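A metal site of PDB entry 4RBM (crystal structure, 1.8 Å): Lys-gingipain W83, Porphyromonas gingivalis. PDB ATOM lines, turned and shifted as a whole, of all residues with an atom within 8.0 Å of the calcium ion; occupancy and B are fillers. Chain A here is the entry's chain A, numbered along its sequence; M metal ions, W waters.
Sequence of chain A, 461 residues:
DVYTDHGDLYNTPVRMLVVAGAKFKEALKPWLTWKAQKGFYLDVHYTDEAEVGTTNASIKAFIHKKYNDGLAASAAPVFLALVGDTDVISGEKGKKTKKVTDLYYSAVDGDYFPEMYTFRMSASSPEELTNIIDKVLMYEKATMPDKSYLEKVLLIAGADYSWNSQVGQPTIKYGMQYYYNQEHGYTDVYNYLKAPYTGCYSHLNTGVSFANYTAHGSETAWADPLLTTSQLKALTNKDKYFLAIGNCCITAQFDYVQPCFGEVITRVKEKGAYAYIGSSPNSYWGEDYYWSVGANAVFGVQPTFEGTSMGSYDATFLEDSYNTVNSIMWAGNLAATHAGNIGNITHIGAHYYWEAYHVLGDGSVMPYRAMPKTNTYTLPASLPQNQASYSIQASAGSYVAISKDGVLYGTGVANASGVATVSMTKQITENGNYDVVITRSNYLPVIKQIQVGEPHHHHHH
OE2 of Glu 115 lies close to N of Val 108.
The backbone NH (N) of Glu 115 sits at hydrogen-bond distance from the backbone carbonyl oxygen (O) of Ser 106, at 2.8 Å.
Along chain A the residues within 4 Å of the calcium ion span positions 109 to 115.
The calcium ion is bound by OD1 of Asp 109 (2.3 Å), O of Phe 113 (2.3 Å), OE1 of Glu 115 (2.3 Å), OD1 of Asp 111 (2.3 Å), water W1 (2.4 Å), water W2 (2.4 Å) and OE2 of Glu 115 (2.6 Å).
The calcium ion has seven donor atoms within binding distance.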
ATOM      1  N   HIS A   6     -23.872  21.970 -12.714  1.00  0.00           N
ATOM      2  CA  HIS A   6     -23.136  21.130 -11.780  1.00  0.00           C
ATOM      3  C   HIS A   6     -21.945  21.884 -11.206  1.00  0.00           C
ATOM      4  O   HIS A   6     -20.797  21.479 -11.388  1.00  0.00           O
ATOM      5  CB  HIS A   6     -22.683  19.828 -12.501  1.00  0.00           C
ATOM      6  CG  HIS A   6     -23.822  19.048 -13.085  1.00  0.00           C
ATOM      7  ND1 HIS A   6     -24.714  18.370 -12.265  1.00  0.00           N
ATOM      8  CD2 HIS A   6     -24.232  18.942 -14.359  1.00  0.00           C
ATOM      9  CE1 HIS A   6     -25.617  17.837 -13.086  1.00  0.00           C
ATOM     10  NE2 HIS A   6     -25.380  18.163 -14.350  1.00  0.00           N
ATOM     11  N   TYR A  67     -27.424   9.536   1.772  1.00  0.00           N
ATOM     12  CA  TYR A  67     -27.517  10.755   0.969  1.00  0.00           C
ATOM     13  C   TYR A  67     -28.980  11.183   0.789  1.00  0.00           C
ATOM     14  O   TYR A  67     -29.325  12.325   1.104  1.00  0.00           O
ATOM     15  CB  TYR A  67     -26.827  10.615  -0.386  1.00  0.00           C
ATOM     16  CG  TYR A  67     -27.005  11.885  -1.190  1.00  0.00           C
ATOM     17  CD1 TYR A  67     -28.063  12.034  -2.083  1.00  0.00           C
ATOM     18  CD2 TYR A  67     -26.204  13.011  -0.935  1.00  0.00           C
ATOM     19  CE1 TYR A  67     -28.315  13.239  -2.714  1.00  0.00           C
ATOM     20  CE2 TYR A  67     -26.447  14.215  -1.577  1.00  0.00           C
ATOM     21  CZ  TYR A  67     -27.489  14.328  -2.482  1.00  0.00           C
ATOM     22  OH  TYR A  67     -27.711  15.503  -3.143  1.00  0.00           O
ATOM     23  N   LEU A 103     -16.627   6.213  -8.254  1.00  0.00           N
ATOM     24  CA  LEU A 103     -17.687   7.099  -8.730  1.00  0.00           C
ATOM     25  C   LEU A 103     -19.086   6.691  -8.262  1.00  0.00           C
ATOM     26  O   LEU A 103     -19.878   7.556  -7.876  1.00  0.00           O
ATOM     27  CB  LEU A 103     -17.701   7.233 -10.271  1.00  0.00           C
ATOM     28  CG  LEU A 103     -18.805   8.169 -10.873  1.00  0.00           C
ATOM     29  CD1 LEU A 103     -18.614   9.661 -10.436  1.00  0.00           C
ATOM     30  CD2 LEU A 103     -18.863   8.037 -12.412  1.00  0.00           C
ATOM     31  N   SER A 106     -20.584   7.808  -4.924  1.00  0.00           N
ATOM     32  CA  SER A 106     -20.965   9.226  -4.888  1.00  0.00           C
ATOM     33  C   SER A 106     -22.098   9.593  -5.838  1.00  0.00           C
ATOM     34  O   SER A 106     -22.743  10.618  -5.649  1.00  0.00           O
ATOM     35  CB  SER A 106     -19.750  10.091  -5.237  1.00  0.00           C
ATOM     36  OG  SER A 106     -19.386   9.980  -6.605  1.00  0.00           O
ATOM     37  N   ALA A 107     -22.265   8.830  -6.917  1.00  0.00           N
ATOM     38  CA  ALA A 107     -23.281   9.090  -7.938  1.00  0.00           C
ATOM     39  C   ALA A 107     -24.573   8.385  -7.513  1.00  0.00           C
ATOM     40  O   ALA A 107     -24.710   7.178  -7.692  1.00  0.00           O
ATOM     41  CB  ALA A 107     -22.776   8.590  -9.297  1.00  0.00           C
ATOM     42  N   VAL A 108     -25.506   9.141  -6.916  1.00  0.00           N
ATOM     43  CA  VAL A 108     -26.719   8.586  -6.316  1.00  0.00           C
ATOM     44  C   VAL A 108     -27.885   8.484  -7.302  1.00  0.00           C
ATOM     45  O   VAL A 108     -28.525   7.436  -7.373  1.00  0.00           O
ATOM     46  CB  VAL A 108     -27.122   9.384  -5.031  1.00  0.00           C
ATOM     47  CG1 VAL A 108     -28.327   8.734  -4.317  1.00  0.00           C
ATOM     48  CG2 VAL A 108     -25.937   9.499  -4.067  1.00  0.00           C
ATOM     49  N   ASP A 109     -28.180   9.568  -8.049  1.00  0.00           N
ATOM     50  CA  ASP A 109     -29.260   9.529  -9.038  1.00  0.00           C
ATOM     51  C   ASP A 109     -28.695   9.013 -10.372  1.00  0.00           C
ATOM     52  O   ASP A 109     -27.571   8.508 -10.402  1.00  0.00           O
ATOM     53  CB  ASP A 109     -29.994  10.884  -9.139  1.00  0.00           C
ATOM     54  CG  ASP A 109     -29.139  12.093  -9.451  1.00  0.00           C
ATOM     55  OD1 ASP A 109     -28.044  11.920 -10.009  1.00  0.00           O
ATOM     56  OD2 ASP A 109     -29.608  13.211  -9.235  1.00  0.00           O
ATOM     57  N   GLY A 110     -29.489   9.097 -11.436  1.00  0.00           N
ATOM     58  CA  GLY A 110     -29.192   8.471 -12.718  1.00  0.00           C
ATOM     59  C   GLY A 110     -28.068   8.949 -13.618  1.00  0.00           C
ATOM     60  O   GLY A 110     -27.685   8.221 -14.537  1.00  0.00           O
ATOM     61  N   ASP A 111     -27.515  10.142 -13.394  1.00  0.00           N
ATOM     62  CA  ASP A 111     -26.468  10.645 -14.287  1.00  0.00           C
ATOM     63  C   ASP A 111     -25.059  10.239 -13.771  1.00  0.00           C
ATOM     64  O   ASP A 111     -24.968   9.493 -12.784  1.00  0.00           O
ATOM     65  CB  ASP A 111     -26.616  12.162 -14.475  1.00  0.00           C
ATOM     66  CG  ASP A 111     -26.494  12.991 -13.203  1.00  0.00           C
ATOM     67  OD1 ASP A 111     -25.843  12.518 -12.247  1.00  0.00           O
ATOM     68  OD2 ASP A 111     -26.928  14.146 -13.202  1.00  0.00           O
ATOM     69  N   TYR A 112     -23.985  10.724 -14.414  1.00  0.00           N
ATOM     70  CA  TYR A 112     -22.625  10.370 -13.990  1.00  0.00           C
ATOM     71  C   TYR A 112     -21.989  11.489 -13.127  1.00  0.00           C
ATOM     72  O   TYR A 112     -20.798  11.410 -12.845  1.00  0.00           O
ATOM     73  CB  TYR A 112     -21.728   9.987 -15.190  1.00  0.00           C
ATOM     74  CG  TYR A 112     -21.675  10.998 -16.326  1.00  0.00           C
ATOM     75  CD1 TYR A 112     -21.088  12.245 -16.151  1.00  0.00           C
ATOM     76  CD2 TYR A 112     -22.141  10.669 -17.592  1.00  0.00           C
ATOM     77  CE1 TYR A 112     -21.009  13.174 -17.194  1.00  0.00           C
ATOM     78  CE2 TYR A 112     -22.025  11.568 -18.658  1.00  0.00           C
ATOM     79  CZ  TYR A 112     -21.478  12.824 -18.453  1.00  0.00           C
ATOM     80  OH  TYR A 112     -21.390  13.725 -19.487  1.00  0.00           O
ATOM     81  N   PHE A 113     -22.779  12.500 -12.707  1.00  0.00           N
ATOM     82  CA  PHE A 113     -22.285  13.562 -11.825  1.00  0.00           C
ATOM     83  C   PHE A 113     -22.453  13.145 -10.365  1.00  0.00           C
ATOM     84  O   PHE A 113     -23.576  12.822  -9.923  1.00  0.00           O
ATOM     85  CB  PHE A 113     -23.004  14.917 -12.082  1.00  0.00           C
ATOM     86  CG  PHE A 113     -22.747  15.461 -13.451  1.00  0.00           C
ATOM     87  CD1 PHE A 113     -21.565  16.144 -13.745  1.00  0.00           C
ATOM     88  CD2 PHE A 113     -23.641  15.222 -14.484  1.00  0.00           C
ATOM     89  CE1 PHE A 113     -21.298  16.604 -15.036  1.00  0.00           C
ATOM     90  CE2 PHE A 113     -23.392  15.695 -15.772  1.00  0.00           C
ATOM     91  CZ  PHE A 113     -22.211  16.380 -16.049  1.00  0.00           C
ATOM     92  N   PRO A 114     -21.373  13.224  -9.566  1.00  0.00           N
ATOM     93  CA  PRO A 114     -21.495  12.870  -8.154  1.00  0.00           C
ATOM     94  C   PRO A 114     -22.447  13.783  -7.392  1.00  0.00           C
ATOM     95  O   PRO A 114     -22.589  14.945  -7.728  1.00  0.00           O
ATOM     96  CB  PRO A 114     -20.061  13.022  -7.622  1.00  0.00           C
ATOM     97  CG  PRO A 114     -19.190  12.893  -8.819  1.00  0.00           C
ATOM     98  CD  PRO A 114     -19.980  13.571  -9.925  1.00  0.00           C
ATOM     99  N   GLU A 115     -23.062  13.273  -6.337  1.00  0.00           N
ATOM    100  CA  GLU A 115     -23.911  14.063  -5.443  1.00  0.00           C
ATOM    101  C   GLU A 115     -23.087  14.588  -4.285  1.00  0.00           C
ATOM    102  O   GLU A 115     -23.501  15.518  -3.609  1.00  0.00           O
ATOM    103  CB  GLU A 115     -25.054  13.165  -4.897  1.00  0.00           C
ATOM    104  CG  GLU A 115     -26.344  13.287  -5.702  1.00  0.00           C
ATOM    105  CD  GLU A 115     -26.154  12.984  -7.175  1.00  0.00           C
ATOM    106  OE1 GLU A 115     -26.067  13.936  -7.987  1.00  0.00           O
ATOM    107  OE2 GLU A 115     -26.037  11.790  -7.527  1.00  0.00           O
ATOM    108  N   MET A 116     -21.936  13.948  -4.032  1.00  0.00           N
ATOM    109  CA  MET A 116     -21.042  14.272  -2.936  1.00  0.00           C
ATOM    110  C   MET A 116     -19.575  14.337  -3.395  1.00  0.00           C
ATOM    111  O   MET A 116     -19.173  13.591  -4.288  1.00  0.00           O
ATOM    112  CB  MET A 116     -21.163  13.199  -1.820  1.00  0.00           C
ATOM    113  CG  MET A 116     -22.530  13.147  -1.141  1.00  0.00           C
ATOM    114  SD  MET A 116     -22.702  11.591  -0.208  1.00  0.00           S
ATOM    115  CE  MET A 116     -22.929  10.452  -1.538  1.00  0.00           C
ATOM    116  N   TRP A 330     -13.099  18.273  -9.507  1.00  0.00           N
ATOM    117  CA  TRP A 330     -14.454  18.548 -10.017  1.00  0.00           C
ATOM    118  C   TRP A 330     -14.376  19.526 -11.205  1.00  0.00           C
ATOM    119  O   TRP A 330     -14.945  19.248 -12.253  1.00  0.00           O
ATOM    120  CB  TRP A 330     -15.294  19.169  -8.890  1.00  0.00           C
ATOM    121  CG  TRP A 330     -16.742  19.333  -9.243  1.00  0.00           C
ATOM    122  CD1 TRP A 330     -17.322  20.380  -9.900  1.00  0.00           C
ATOM    123  CD2 TRP A 330     -17.776  18.392  -8.985  1.00  0.00           C
ATOM    124  NE1 TRP A 330     -18.671  20.164 -10.044  1.00  0.00           N
ATOM    125  CE2 TRP A 330     -18.985  18.946  -9.494  1.00  0.00           C
ATOM    126  CE3 TRP A 330     -17.822  17.150  -8.341  1.00  0.00           C
ATOM    127  CZ2 TRP A 330     -20.219  18.288  -9.359  1.00  0.00           C
ATOM    128  CZ3 TRP A 330     -19.048  16.505  -8.218  1.00  0.00           C
ATOM    129  CH2 TRP A 330     -20.220  17.067  -8.741  1.00  0.00           C
HETATM  130 CA    CA M   1     -25.884  12.670  -9.922  1.00  0.00          CA
HETATM  131  O   HOH W   1     -26.342  14.836 -10.860  1.00  0.00           O
HETATM  132  O   HOH W   2     -25.450  10.282 -10.149  1.00  0.00           O
